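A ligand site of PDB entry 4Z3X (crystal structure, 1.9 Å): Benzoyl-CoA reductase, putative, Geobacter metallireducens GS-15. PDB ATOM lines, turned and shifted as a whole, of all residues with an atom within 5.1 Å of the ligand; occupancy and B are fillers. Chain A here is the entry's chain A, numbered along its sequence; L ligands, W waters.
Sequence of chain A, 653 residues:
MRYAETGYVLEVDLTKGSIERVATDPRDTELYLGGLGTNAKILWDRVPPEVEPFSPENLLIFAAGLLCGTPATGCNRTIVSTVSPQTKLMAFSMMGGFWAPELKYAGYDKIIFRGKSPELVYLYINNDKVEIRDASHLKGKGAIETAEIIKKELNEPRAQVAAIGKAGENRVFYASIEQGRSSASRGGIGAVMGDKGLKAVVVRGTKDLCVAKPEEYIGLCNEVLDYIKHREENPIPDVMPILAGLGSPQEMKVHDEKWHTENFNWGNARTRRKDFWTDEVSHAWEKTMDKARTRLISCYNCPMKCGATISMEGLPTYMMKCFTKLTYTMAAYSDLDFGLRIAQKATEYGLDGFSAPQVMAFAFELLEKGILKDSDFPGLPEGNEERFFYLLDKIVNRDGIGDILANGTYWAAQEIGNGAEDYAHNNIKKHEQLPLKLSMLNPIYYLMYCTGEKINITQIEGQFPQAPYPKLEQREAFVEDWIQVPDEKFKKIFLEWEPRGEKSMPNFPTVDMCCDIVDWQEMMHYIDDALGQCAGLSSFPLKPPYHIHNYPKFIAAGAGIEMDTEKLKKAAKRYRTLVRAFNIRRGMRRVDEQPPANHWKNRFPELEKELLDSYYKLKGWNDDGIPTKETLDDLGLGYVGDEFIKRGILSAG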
ATOM      1  N   ILE A 242     -17.200 -24.744  22.160  1.00  0.00           N
ATOM      2  CA  ILE A 242     -17.653 -25.502  20.980  1.00  0.00           C
ATOM      3  C   ILE A 242     -17.655 -24.636  19.708  1.00  0.00           C
ATOM      4  O   ILE A 242     -17.430 -25.171  18.625  1.00  0.00           O
ATOM      5  CB  ILE A 242     -19.067 -26.140  21.145  1.00  0.00           C
ATOM      6  CG1 ILE A 242     -20.159 -25.087  21.022  1.00  0.00           C
ATOM      7  CG2 ILE A 242     -19.182 -26.997  22.428  1.00  0.00           C
ATOM      8  CD1 ILE A 242     -21.483 -25.678  20.639  1.00  0.00           C
ATOM      9  N   LEU A 243     -17.768 -23.313  19.845  1.00  0.00           N
ATOM     10  CA  LEU A 243     -17.759 -22.414  18.688  1.00  0.00           C
ATOM     11  C   LEU A 243     -16.638 -21.370  18.615  1.00  0.00           C
ATOM     12  O   LEU A 243     -16.611 -20.592  17.653  1.00  0.00           O
ATOM     13  CB  LEU A 243     -19.103 -21.665  18.636  1.00  0.00           C
ATOM     14  CG  LEU A 243     -20.327 -22.596  18.521  1.00  0.00           C
ATOM     15  CD1 LEU A 243     -21.674 -21.856  18.621  1.00  0.00           C
ATOM     16  CD2 LEU A 243     -20.266 -23.450  17.229  1.00  0.00           C
ATOM     17  N   PRO A 249     -18.687 -27.644  14.809  1.00  0.00           N
ATOM     18  CA  PRO A 249     -18.833 -27.471  16.278  1.00  0.00           C
ATOM     19  C   PRO A 249     -18.091 -28.560  17.078  1.00  0.00           C
ATOM     20  O   PRO A 249     -18.305 -29.770  16.886  1.00  0.00           O
ATOM     21  CB  PRO A 249     -20.355 -27.574  16.460  1.00  0.00           C
ATOM     22  CG  PRO A 249     -20.843 -26.923  15.281  1.00  0.00           C
ATOM     23  CD  PRO A 249     -19.968 -27.425  14.141  1.00  0.00           C
ATOM     24  N   GLU A 251     -18.059 -30.367  19.518  1.00  0.00           N
ATOM     25  CA  GLU A 251     -18.832 -31.107  20.522  1.00  0.00           C
ATOM     26  C   GLU A 251     -18.215 -32.442  20.991  1.00  0.00           C
ATOM     27  O   GLU A 251     -18.489 -32.928  22.090  1.00  0.00           O
ATOM     28  CB  GLU A 251     -20.237 -31.362  19.956  1.00  0.00           C
ATOM     29  CG  GLU A 251     -21.072 -30.056  20.070  1.00  0.00           C
ATOM     30  CD  GLU A 251     -22.502 -30.285  19.773  1.00  0.00           C
ATOM     31  OE1 GLU A 251     -22.871 -30.081  18.602  1.00  0.00           O
ATOM     32  OE2 GLU A 251     -23.249 -30.670  20.701  1.00  0.00           O
ATOM     33  N   TRP A 259     -25.086 -24.344  26.903  1.00  0.00           N
ATOM     34  CA  TRP A 259     -25.685 -23.489  25.910  1.00  0.00           C
ATOM     35  C   TRP A 259     -26.761 -24.262  25.142  1.00  0.00           C
ATOM     36  O   TRP A 259     -27.891 -23.798  25.043  1.00  0.00           O
ATOM     37  CB  TRP A 259     -24.607 -22.941  24.959  1.00  0.00           C
ATOM     38  CG  TRP A 259     -25.096 -21.925  23.945  1.00  0.00           C
ATOM     39  CD1 TRP A 259     -25.448 -20.623  24.186  1.00  0.00           C
ATOM     40  CD2 TRP A 259     -25.267 -22.131  22.533  1.00  0.00           C
ATOM     41  NE1 TRP A 259     -25.834 -20.025  23.008  1.00  0.00           N
ATOM     42  CE2 TRP A 259     -25.745 -20.922  21.982  1.00  0.00           C
ATOM     43  CE3 TRP A 259     -25.082 -23.224  21.676  1.00  0.00           C
ATOM     44  CZ2 TRP A 259     -25.992 -20.763  20.626  1.00  0.00           C
ATOM     45  CZ3 TRP A 259     -25.350 -23.071  20.322  1.00  0.00           C
ATOM     46  CH2 TRP A 259     -25.799 -21.844  19.809  1.00  0.00           C
ATOM     47  N   HIS A 260     -26.396 -25.451  24.633  1.00  0.00           N
ATOM     48  CA  HIS A 260     -27.346 -26.301  23.938  1.00  0.00           C
ATOM     49  C   HIS A 260     -28.545 -26.744  24.781  1.00  0.00           C
ATOM     50  O   HIS A 260     -29.691 -26.532  24.368  1.00  0.00           O
ATOM     51  CB  HIS A 260     -26.660 -27.545  23.380  1.00  0.00           C
ATOM     52  CG  HIS A 260     -25.979 -27.316  22.083  1.00  0.00           C
ATOM     53  ND1 HIS A 260     -24.697 -27.758  21.832  1.00  0.00           N
ATOM     54  CD2 HIS A 260     -26.381 -26.664  20.967  1.00  0.00           C
ATOM     55  CE1 HIS A 260     -24.352 -27.410  20.599  1.00  0.00           C
ATOM     56  NE2 HIS A 260     -25.364 -26.735  20.060  1.00  0.00           N
ATOM     57  N   ASN A 263     -30.832 -23.631  26.016  1.00  0.00           N
ATOM     58  CA  ASN A 263     -31.371 -22.705  25.036  1.00  0.00           C
ATOM     59  C   ASN A 263     -32.130 -23.411  23.913  1.00  0.00           C
ATOM     60  O   ASN A 263     -32.986 -22.801  23.306  1.00  0.00           O
ATOM     61  CB  ASN A 263     -30.247 -21.849  24.438  1.00  0.00           C
ATOM     62  CG  ASN A 263     -29.746 -20.797  25.402  1.00  0.00           C
ATOM     63  OD1 ASN A 263     -30.524 -20.243  26.146  1.00  0.00           O
ATOM     64  ND2 ASN A 263     -28.440 -20.537  25.397  1.00  0.00           N
ATOM     65  N   PHE A 264     -31.820 -24.698  23.656  1.00  0.00           N
ATOM     66  CA  PHE A 264     -32.540 -25.465  22.636  1.00  0.00           C
ATOM     67  C   PHE A 264     -33.732 -26.234  23.232  1.00  0.00           C
ATOM     68  O   PHE A 264     -33.757 -26.581  24.391  1.00  0.00           O
ATOM     69  CB  PHE A 264     -31.592 -26.411  21.889  1.00  0.00           C
ATOM     70  CG  PHE A 264     -30.676 -25.703  20.904  1.00  0.00           C
ATOM     71  CD1 PHE A 264     -29.788 -24.710  21.358  1.00  0.00           C
ATOM     72  CD2 PHE A 264     -30.680 -26.037  19.580  1.00  0.00           C
ATOM     73  CE1 PHE A 264     -28.940 -24.079  20.460  1.00  0.00           C
ATOM     74  CE2 PHE A 264     -29.810 -25.422  18.683  1.00  0.00           C
ATOM     75  CZ  PHE A 264     -28.968 -24.434  19.110  1.00  0.00           C
ATOM     76  N   ARG A 272     -38.424 -25.750  26.588  1.00  0.00           N
ATOM     77  CA  ARG A 272     -37.199 -25.119  27.134  1.00  0.00           C
ATOM     78  C   ARG A 272     -36.979 -25.514  28.589  1.00  0.00           C
ATOM     79  O   ARG A 272     -37.873 -25.363  29.408  1.00  0.00           O
ATOM     80  CB  ARG A 272     -37.225 -23.583  27.042  1.00  0.00           C
ATOM     81  CG  ARG A 272     -35.792 -22.928  26.961  1.00  0.00           C
ATOM     82  CD  ARG A 272     -35.814 -21.426  27.245  1.00  0.00           C
ATOM     83  NE  ARG A 272     -34.626 -20.677  26.823  1.00  0.00           N
ATOM     84  CZ  ARG A 272     -34.404 -20.234  25.568  1.00  0.00           C
ATOM     85  NH1 ARG A 272     -35.288 -20.494  24.587  1.00  0.00           N
ATOM     86  NH2 ARG A 272     -33.296 -19.542  25.276  1.00  0.00           N
ATOM     87  N   CYS A 322     -20.324 -33.180  15.792  1.00  0.00           N
ATOM     88  CA  CYS A 322     -21.365 -32.144  15.866  1.00  0.00           C
ATOM     89  C   CYS A 322     -22.656 -32.575  16.587  1.00  0.00           C
ATOM     90  O   CYS A 322     -22.628 -33.323  17.595  1.00  0.00           O
ATOM     91  CB  CYS A 322     -21.705 -31.650  14.439  1.00  0.00           C
ATOM     92  SG  CYS A 322     -22.485 -30.005  14.329  1.00  0.00           S
ATOM     93  N   PHE A 323     -23.803 -32.046  16.110  1.00  0.00           N
ATOM     94  CA  PHE A 323     -24.946 -31.955  17.011  1.00  0.00           C
ATOM     95  C   PHE A 323     -25.745 -33.261  17.192  1.00  0.00           C
ATOM     96  O   PHE A 323     -26.592 -33.318  18.081  1.00  0.00           O
ATOM     97  CB  PHE A 323     -25.877 -30.810  16.510  1.00  0.00           C
ATOM     98  CG  PHE A 323     -26.917 -30.361  17.492  1.00  0.00           C
ATOM     99  CD1 PHE A 323     -26.604 -30.108  18.830  1.00  0.00           C
ATOM    100  CD2 PHE A 323     -28.231 -30.092  17.054  1.00  0.00           C
ATOM    101  CE1 PHE A 323     -27.613 -29.657  19.717  1.00  0.00           C
ATOM    102  CE2 PHE A 323     -29.223 -29.630  17.951  1.00  0.00           C
ATOM    103  CZ  PHE A 323     -28.907 -29.433  19.274  1.00  0.00           C
ATOM    104  N   LEU A 434     -33.794 -26.978  13.038  1.00  0.00           N
ATOM    105  CA  LEU A 434     -33.274 -27.039  14.431  1.00  0.00           C
ATOM    106  C   LEU A 434     -34.362 -26.769  15.495  1.00  0.00           C
ATOM    107  O   LEU A 434     -35.307 -25.926  15.304  1.00  0.00           O
ATOM    108  CB  LEU A 434     -32.106 -26.071  14.638  1.00  0.00           C
ATOM    109  CG  LEU A 434     -30.697 -26.517  14.211  1.00  0.00           C
ATOM    110  CD1 LEU A 434     -30.113 -27.539  15.145  1.00  0.00           C
ATOM    111  CD2 LEU A 434     -30.768 -27.076  12.815  1.00  0.00           C
ATOM    112  N   LEU A 436     -35.226 -24.910  17.923  1.00  0.00           N
ATOM    113  CA  LEU A 436     -34.960 -23.575  18.500  1.00  0.00           C
ATOM    114  C   LEU A 436     -36.207 -22.720  18.419  1.00  0.00           C
ATOM    115  O   LEU A 436     -36.687 -22.473  17.296  1.00  0.00           O
ATOM    116  CB  LEU A 436     -33.883 -22.866  17.687  1.00  0.00           C
ATOM    117  CG  LEU A 436     -32.410 -22.905  17.928  1.00  0.00           C
ATOM    118  CD1 LEU A 436     -31.772 -22.630  16.567  1.00  0.00           C
ATOM    119  CD2 LEU A 436     -32.049 -21.849  18.970  1.00  0.00           C
ATOM    120  N   LEU A 438     -37.196 -19.151  19.960  1.00  0.00           N
ATOM    121  CA  LEU A 438     -36.622 -18.012  20.685  1.00  0.00           C
ATOM    122  C   LEU A 438     -37.648 -16.899  20.907  1.00  0.00           C
ATOM    123  O   LEU A 438     -38.769 -16.969  20.403  1.00  0.00           O
ATOM    124  CB  LEU A 438     -35.425 -17.496  19.909  1.00  0.00           C
ATOM    125  CG  LEU A 438     -34.311 -18.590  19.802  1.00  0.00           C
ATOM    126  CD1 LEU A 438     -33.133 -18.090  19.008  1.00  0.00           C
ATOM    127  CD2 LEU A 438     -33.886 -19.102  21.175  1.00  0.00           C
ATOM    128  N   SER A 439     -37.281 -15.884  21.686  1.00  0.00           N
ATOM    129  CA  SER A 439     -38.238 -14.871  22.116  1.00  0.00           C
ATOM    130  C   SER A 439     -38.343 -13.726  21.117  1.00  0.00           C
ATOM    131  O   SER A 439     -39.419 -13.422  20.644  1.00  0.00           O
ATOM    132  CB  SER A 439     -37.868 -14.323  23.509  1.00  0.00           C
ATOM    133  OG  SER A 439     -38.740 -13.247  23.841  1.00  0.00           O
ATOM    134  N   MET A 440     -37.223 -13.115  20.758  1.00  0.00           N
ATOM    135  CA  MET A 440     -37.251 -11.917  19.920  1.00  0.00           C
ATOM    136  C   MET A 440     -36.873 -12.215  18.468  1.00  0.00           C
ATOM    137  O   MET A 440     -35.890 -12.861  18.214  1.00  0.00           O
ATOM    138  CB  MET A 440     -36.332 -10.851  20.531  1.00  0.00           C
ATOM    139  CG  MET A 440     -36.298  -9.552  19.777  1.00  0.00           C
ATOM    140  SD  MET A 440     -37.895  -8.694  19.940  1.00  0.00           S
ATOM    141  CE  MET A 440     -38.053  -8.522  21.729  1.00  0.00           C
ATOM    142  N   ASN A 442     -35.182 -12.252  15.145  1.00  0.00           N
ATOM    143  CA  ASN A 442     -33.821 -11.924  14.750  1.00  0.00           C
ATOM    144  C   ASN A 442     -33.901 -11.726  13.235  1.00  0.00           C
ATOM    145  O   ASN A 442     -34.205 -12.654  12.496  1.00  0.00           O
ATOM    146  CB  ASN A 442     -32.833 -13.068  15.183  1.00  0.00           C
ATOM    147  CG  ASN A 442     -31.400 -12.812  14.752  1.00  0.00           C
ATOM    148  OD1 ASN A 442     -31.135 -12.326  13.657  1.00  0.00           O
ATOM    149  ND2 ASN A 442     -30.440 -13.157  15.650  1.00  0.00           N
ATOM    150  N   TYR A 445     -31.433 -13.889  11.014  1.00  0.00           N
ATOM    151  CA  TYR A 445     -31.892 -15.280  11.001  1.00  0.00           C
ATOM    152  C   TYR A 445     -33.190 -15.472  10.221  1.00  0.00           C
ATOM    153  O   TYR A 445     -33.343 -16.470   9.472  1.00  0.00           O
ATOM    154  CB  TYR A 445     -31.987 -15.804  12.447  1.00  0.00           C
ATOM    155  CG  TYR A 445     -30.587 -16.292  12.828  1.00  0.00           C
ATOM    156  CD1 TYR A 445     -29.579 -15.383  13.139  1.00  0.00           C
ATOM    157  CD2 TYR A 445     -30.235 -17.659  12.724  1.00  0.00           C
ATOM    158  CE1 TYR A 445     -28.286 -15.796  13.414  1.00  0.00           C
ATOM    159  CE2 TYR A 445     -28.952 -18.084  13.025  1.00  0.00           C
ATOM    160  CZ  TYR A 445     -27.983 -17.142  13.371  1.00  0.00           C
ATOM    161  OH  TYR A 445     -26.667 -17.536  13.648  1.00  0.00           O
ATOM    162  N   TYR A 449     -33.530 -18.402   7.441  1.00  0.00           N
ATOM    163  CA  TYR A 449     -34.573 -19.401   7.471  1.00  0.00           C
ATOM    164  C   TYR A 449     -35.494 -19.332   6.211  1.00  0.00           C
ATOM    165  O   TYR A 449     -35.837 -20.365   5.642  1.00  0.00           O
ATOM    166  CB  TYR A 449     -35.456 -19.265   8.701  1.00  0.00           C
ATOM    167  CG  TYR A 449     -34.870 -19.717   9.995  1.00  0.00           C
ATOM    168  CD1 TYR A 449     -34.550 -21.075  10.215  1.00  0.00           C
ATOM    169  CD2 TYR A 449     -34.652 -18.807  11.037  1.00  0.00           C
ATOM    170  CE1 TYR A 449     -34.011 -21.500  11.434  1.00  0.00           C
ATOM    171  CE2 TYR A 449     -34.116 -19.224  12.251  1.00  0.00           C
ATOM    172  CZ  TYR A 449     -33.781 -20.575  12.434  1.00  0.00           C
ATOM    173  OH  TYR A 449     -33.258 -20.973  13.667  1.00  0.00           O
ATOM    174  N   ILE A 457     -30.441 -24.041   8.913  1.00  0.00           N
ATOM    175  CA  ILE A 457     -29.759 -22.871   9.472  1.00  0.00           C
ATOM    176  C   ILE A 457     -28.260 -23.073   9.789  1.00  0.00           C
ATOM    177  O   ILE A 457     -27.469 -22.123   9.651  1.00  0.00           O
ATOM    178  CB  ILE A 457     -30.546 -22.385  10.727  1.00  0.00           C
ATOM    179  CG1 ILE A 457     -30.306 -20.874  11.023  1.00  0.00           C
ATOM    180  CG2 ILE A 457     -30.284 -23.282  11.962  1.00  0.00           C
ATOM    181  CD1 ILE A 457     -30.802 -19.943   9.902  1.00  0.00           C
ATOM    182  N   THR A 458     -27.822 -24.287  10.141  1.00  0.00           N
ATOM    183  CA  THR A 458     -26.427 -24.437  10.496  1.00  0.00           C
ATOM    184  C   THR A 458     -25.572 -24.484   9.231  1.00  0.00           C
ATOM    185  O   THR A 458     -24.357 -24.440   9.287  1.00  0.00           O
ATOM    186  CB  THR A 458     -26.124 -25.690  11.372  1.00  0.00           C
ATOM    187  OG1 THR A 458     -26.353 -26.863  10.624  1.00  0.00           O
ATOM    188  CG2 THR A 458     -27.002 -25.761  12.587  1.00  0.00           C
ATOM    189  N   GLU A 461     -25.368 -19.974   8.089  1.00  0.00           N
ATOM    190  CA  GLU A 461     -24.726 -18.996   8.999  1.00  0.00           C
ATOM    191  C   GLU A 461     -23.179 -19.108   9.072  1.00  0.00           C
ATOM    192  O   GLU A 461     -22.555 -19.985   8.484  1.00  0.00           O
ATOM    193  CB  GLU A 461     -25.257 -19.168  10.447  1.00  0.00           C
ATOM    194  CG  GLU A 461     -24.561 -20.409  11.126  1.00  0.00           C
ATOM    195  CD  GLU A 461     -25.249 -20.827  12.428  1.00  0.00           C
ATOM    196  OE1 GLU A 461     -26.078 -20.066  12.934  1.00  0.00           O
ATOM    197  OE2 GLU A 461     -24.941 -21.910  12.973  1.00  0.00           O
ATOM    198  N   GLN A 466     -22.923 -14.313  15.870  1.00  0.00           N
ATOM    199  CA  GLN A 466     -24.342 -14.565  16.239  1.00  0.00           C
ATOM    200  C   GLN A 466     -24.988 -13.546  17.197  1.00  0.00           C
ATOM    201  O   GLN A 466     -26.201 -13.529  17.331  1.00  0.00           O
ATOM    202  CB  GLN A 466     -24.486 -15.961  16.877  1.00  0.00           C
ATOM    203  CG  GLN A 466     -24.417 -17.134  15.895  1.00  0.00           C
ATOM    204  CD  GLN A 466     -24.966 -18.437  16.479  1.00  0.00           C
ATOM    205  OE1 GLN A 466     -25.802 -18.408  17.369  1.00  0.00           O
ATOM    206  NE2 GLN A 466     -24.466 -19.574  15.974  1.00  0.00           N
ATOM    207  N   PRO A 499     -26.288  -5.450  22.430  1.00  0.00           N
ATOM    208  CA  PRO A 499     -27.266  -6.395  23.007  1.00  0.00           C
ATOM    209  C   PRO A 499     -28.573  -5.741  23.396  1.00  0.00           C
ATOM    210  O   PRO A 499     -29.624  -6.358  23.163  1.00  0.00           O
ATOM    211  CB  PRO A 499     -26.567  -6.935  24.256  1.00  0.00           C
ATOM    212  CG  PRO A 499     -25.392  -6.031  24.452  1.00  0.00           C
ATOM    213  CD  PRO A 499     -25.011  -5.481  23.139  1.00  0.00           C
ATOM    214  N   ARG A 500     -28.508  -4.524  23.968  1.00  0.00           N
ATOM    215  CA  ARG A 500     -29.689  -3.769  24.411  1.00  0.00           C
ATOM    216  C   ARG A 500     -29.623  -2.313  24.003  1.00  0.00           C
ATOM    217  O   ARG A 500     -28.551  -1.705  23.957  1.00  0.00           O
ATOM    218  CB  ARG A 500     -29.858  -3.864  25.920  1.00  0.00           C
ATOM    219  CG  ARG A 500     -30.094  -5.257  26.483  1.00  0.00           C
ATOM    220  CD  ARG A 500     -31.497  -5.748  26.146  1.00  0.00           C
ATOM    221  NE  ARG A 500     -31.815  -7.048  26.748  1.00  0.00           N
ATOM    222  CZ  ARG A 500     -31.684  -8.225  26.146  1.00  0.00           C
ATOM    223  NH1 ARG A 500     -31.210  -8.299  24.897  1.00  0.00           N
ATOM    224  NH2 ARG A 500     -32.023  -9.348  26.778  1.00  0.00           N
ATOM    225  N   SER A 504     -30.140  -2.289  19.149  1.00  0.00           N
ATOM    226  CA  SER A 504     -30.338  -3.719  19.353  1.00  0.00           C
ATOM    227  C   SER A 504     -31.384  -4.308  18.351  1.00  0.00           C
ATOM    228  O   SER A 504     -32.154  -3.582  17.739  1.00  0.00           O
ATOM    229  CB  SER A 504     -30.747  -3.989  20.798  1.00  0.00           C
ATOM    230  OG  SER A 504     -32.084  -3.575  21.029  1.00  0.00           O
ATOM    231  N   MET A 505     -31.405  -5.624  18.167  1.00  0.00           N
ATOM    232  CA  MET A 505     -32.477  -6.240  17.341  1.00  0.00           C
ATOM    233  C   MET A 505     -33.880  -6.061  18.004  1.00  0.00           C
ATOM    234  O   MET A 505     -33.977  -5.966  19.228  1.00  0.00           O
ATOM    235  CB  MET A 505     -32.173  -7.714  17.113  1.00  0.00           C
ATOM    236  CG  MET A 505     -30.885  -7.969  16.349  1.00  0.00           C
ATOM    237  SD  MET A 505     -30.558  -9.744  16.163  1.00  0.00           S
ATOM    238  CE  MET A 505     -29.485  -9.634  14.709  1.00  0.00           C
ATOM    239  N   PHE A 540     -17.993 -21.668   8.098  1.00  0.00           N
ATOM    240  CA  PHE A 540     -18.744 -21.865   9.341  1.00  0.00           C
ATOM    241  C   PHE A 540     -18.203 -21.066  10.569  1.00  0.00           C
ATOM    242  O   PHE A 540     -18.979 -20.359  11.205  1.00  0.00           O
ATOM    243  CB  PHE A 540     -18.864 -23.324   9.685  1.00  0.00           C
ATOM    244  CG  PHE A 540     -19.702 -23.579  10.932  1.00  0.00           C
ATOM    245  CD1 PHE A 540     -19.131 -23.540  12.204  1.00  0.00           C
ATOM    246  CD2 PHE A 540     -21.071 -23.835  10.808  1.00  0.00           C
ATOM    247  CE1 PHE A 540     -19.887 -23.795  13.346  1.00  0.00           C
ATOM    248  CE2 PHE A 540     -21.852 -24.065  11.944  1.00  0.00           C
ATOM    249  CZ  PHE A 540     -21.272 -24.026  13.212  1.00  0.00           C
ATOM    250  N   ASN A 602     -42.115 -13.007  19.650  1.00  0.00           N
ATOM    251  CA  ASN A 602     -42.384 -11.623  19.282  1.00  0.00           C
ATOM    252  C   ASN A 602     -42.165 -11.504  17.811  1.00  0.00           C
ATOM    253  O   ASN A 602     -41.027 -11.685  17.381  1.00  0.00           O
ATOM    254  CB  ASN A 602     -41.442 -10.627  20.010  1.00  0.00           C
ATOM    255  CG  ASN A 602     -41.672 -10.557  21.486  1.00  0.00           C
ATOM    256  OD1 ASN A 602     -41.143 -11.364  22.243  1.00  0.00           O
ATOM    257  ND2 ASN A 602     -42.391  -9.553  21.927  1.00  0.00           N
HETATM  258  N1  LIG L   1     -34.153  -5.670  24.241  1.00  0.00           N
HETATM  259  O1  LIG L   1     -34.663 -14.241  21.777  1.00  0.00           O
HETATM  260  P1  LIG L   1     -34.029 -14.638  23.102  1.00  0.00           P
HETATM  261  C1  LIG L   1     -26.472 -23.292  15.797  1.00  0.00           C
HETATM  262  C2  LIG L   1     -35.286 -10.550  25.613  1.00  0.00           C
HETATM  263  S1  LIG L   1     -28.227 -23.238  15.431  1.00  0.00           S
HETATM  264  C3  LIG L   1     -34.713  -6.175  25.346  1.00  0.00           C
HETATM  265  O2  LIG L   1     -34.725 -15.819  23.683  1.00  0.00           O
HETATM  266  P2  LIG L   1     -31.296 -15.239  23.894  1.00  0.00           P
HETATM  267  C4  LIG L   1     -25.905 -24.567  16.208  1.00  0.00           C
HETATM  268  C5  LIG L   1     -36.287 -11.568  25.086  1.00  0.00           C
HETATM  269  O3  LIG L   1     -37.617 -11.076  25.010  1.00  0.00           O
HETATM  270  C6  LIG L   1     -28.496 -21.444  15.392  1.00  0.00           C
HETATM  271  N2  LIG L   1     -35.014  -7.441  25.641  1.00  0.00           N
HETATM  272  O4  LIG L   1     -32.471 -14.810  22.897  1.00  0.00           O
HETATM  273  C7  LIG L   1     -24.397 -24.577  16.294  1.00  0.00           C
HETATM  274  C8  LIG L   1     -36.164 -12.637  26.168  1.00  0.00           C
HETATM  275  O5  LIG L   1     -36.821 -12.251  27.390  1.00  0.00           O
HETATM  276  P3  LIG L   1     -37.763 -13.117  28.341  1.00  0.00           P
HETATM  277  C9  LIG L   1     -28.325 -20.762  16.747  1.00  0.00           C
HETATM  278  C10 LIG L   1     -34.669  -8.265  24.638  1.00  0.00           C
HETATM  279  O6  LIG L   1     -30.682 -14.064  24.496  1.00  0.00           O
HETATM  280  C11 LIG L   1     -23.837 -25.966  16.068  1.00  0.00           C
HETATM  281  C12 LIG L   1     -34.658 -12.652  26.455  1.00  0.00           C
HETATM  282  O7  LIG L   1     -34.212 -11.308  26.141  1.00  0.00           O
HETATM  283  N3  LIG L   1     -28.428 -19.320  16.587  1.00  0.00           N
HETATM  284  O8  LIG L   1     -25.753 -22.322  15.627  1.00  0.00           O
HETATM  285  O9  LIG L   1     -31.882 -16.335  24.888  1.00  0.00           O
HETATM  286  C13 LIG L   1     -24.529 -27.045  16.890  1.00  0.00           C
HETATM  287  C14 LIG L   1     -33.887 -13.651  25.619  1.00  0.00           C
HETATM  288  O10 LIG L   1     -34.099 -13.388  24.200  1.00  0.00           O
HETATM  289  C15 LIG L   1     -34.108  -7.896  23.418  1.00  0.00           C
HETATM  290  C16 LIG L   1     -29.631 -18.726  16.523  1.00  0.00           C
HETATM  291  O11 LIG L   1     -30.676 -19.370  16.555  1.00  0.00           O
HETATM  292  C17 LIG L   1     -33.839  -6.524  23.221  1.00  0.00           C
HETATM  293  N4  LIG L   1     -33.306  -6.022  22.104  1.00  0.00           N
HETATM  294  O12 LIG L   1     -30.325 -15.663  22.679  1.00  0.00           O
HETATM  295  C18 LIG L   1     -26.019 -27.074  16.496  1.00  0.00           C
HETATM  296  C19 LIG L   1     -29.649 -17.213  16.469  1.00  0.00           C
HETATM  297  N5  LIG L   1     -33.873  -9.013  22.619  1.00  0.00           N
HETATM  298  O13 LIG L   1     -38.666 -13.980  27.514  1.00  0.00           O
HETATM  299  C20 LIG L   1     -26.626 -25.696  16.372  1.00  0.00           C
HETATM  300  C21 LIG L   1     -28.397 -16.591  17.049  1.00  0.00           C
HETATM  301  C22 LIG L   1     -34.280 -10.008  23.365  1.00  0.00           C
HETATM  302  O14 LIG L   1     -38.529 -12.097  29.212  1.00  0.00           O
HETATM  303  N6  LIG L   1     -28.159 -17.036  18.426  1.00  0.00           N
HETATM  304  N7  LIG L   1     -34.771  -9.637  24.584  1.00  0.00           N
HETATM  305  O15 LIG L   1     -36.821 -13.879  29.262  1.00  0.00           O
HETATM  306  C23 LIG L   1     -28.661 -16.354  19.446  1.00  0.00           C
HETATM  307  O16 LIG L   1     -29.535 -15.509  19.286  1.00  0.00           O
HETATM  308  C24 LIG L   1     -28.141 -16.689  20.834  1.00  0.00           C
HETATM  309  O17 LIG L   1     -26.954 -17.513  20.791  1.00  0.00           O
HETATM  310  C25 LIG L   1     -29.281 -17.491  21.493  1.00  0.00           C
HETATM  311  C26 LIG L   1     -30.546 -16.659  21.673  1.00  0.00           C
HETATM  312  C27 LIG L   1     -28.794 -17.953  22.881  1.00  0.00           C
HETATM  313  C28 LIG L   1     -29.643 -18.707  20.630  1.00  0.00           C
HETATM  314  O   HOH W   1     -33.648 -13.699  19.525  1.00  0.00           O
HETATM  315  O   HOH W   2     -31.695 -14.841  17.570  1.00  0.00           O
HETATM  316  O   HOH W   3     -33.302 -19.264  15.377  1.00  0.00           O
HETATM  317  O   HOH W   4     -33.225  -2.745  23.784  1.00  0.00           O
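The backbone carbonyl oxygen (O) of Trp 259 sits close to the side-chain amide nitrogen (ND2) of Asn 263, at 3.3 Å.
The side-chain carboxylate (OE1) of Glu 251 lies close to the backbone NH (N) of Phe 323, at 3.3 Å.
The backbone NH of Asn 602 is in hydrogen-bond range of the backbone carbonyl oxygen of Ser 439 (2.9 Å).
NH2 of Arg 272 is in hydrogen-bond range of OD1 of Asn 263 (3.0 Å).
The side-chain hydroxyl (OH) of Tyr 445 lies within hydrogen-bond range of the side-chain carboxylate (OE1) of Glu 461 (2.7 Å).
The backbone NH (N) of Tyr 445 lies within hydrogen-bond range of the side-chain amide oxygen (OD1) of Asn 442.
OE2 of Glu 251 lies within hydrogen-bond range of ND1 of His 260, 3.4 Å away.
The side-chain amide nitrogen (ND2) of Asn 442 is in hydrogen-bond range of the side-chain sulfur (SD) of Met 505, 3.5 Å away.
Water W1 bridges an oxygen (O1) of the ligand (2.5 Å) and the backbone carbonyl oxygen (O) of Met 440 (2.7 Å).
Water W2 bridges an oxygen (O16) of the ligand and the side-chain amide nitrogen of Asn 442.
Water W3 bridges OH of Tyr 449 (2.4 Å) and O11 of the ligand (2.9 Å).
Water W4 lies within hydrogen-bond range of OG of Ser 504 and N1 of the ligand.
OE2 of Glu 461 lies close to O8 of the ligand, 2.8 Å away.
Residues that only touch the ligand: Pro 249, Glu 251, Trp 259, His 260, Asn 263, Phe 264, Phe 323, Leu 436, Leu 438, Tyr 445, Thr 458 and Pro 499.
Of the 29 residues printed, 20 come within 4 Å of the ligand.
The nearest printed residue that does not touch the ligand is Ile 457 (4.03 Å).
The side-chain hydroxyl (OG) of Ser 439 lies within hydrogen-bond range of an oxygen (O3) of the ligand (2.7 Å).
NH2 of Arg 500 is in hydrogen-bond range of O7 of the ligand (3.0 Å).
N4 of the ligand lies within hydrogen-bond range of O of Met 505 (3.0 Å).
NH2 of Arg 272 is in salt-bridge range of O9 of the ligand, 3.5 Å away.
An oxygen (O1) of the ligand is in hydrogen-bond range of the backbone NH (N) of Met 440.
N3 of the ligand lies within hydrogen-bond range of OE1 of Gln 466 (2.9 Å).
The side-chain hydroxyl (OG) of Ser 504 lies within hydrogen-bond range of a nitrogen (N4) of the ligand (2.9 Å).
N of Ser 439 lies within hydrogen-bond range of O1 of the ligand.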
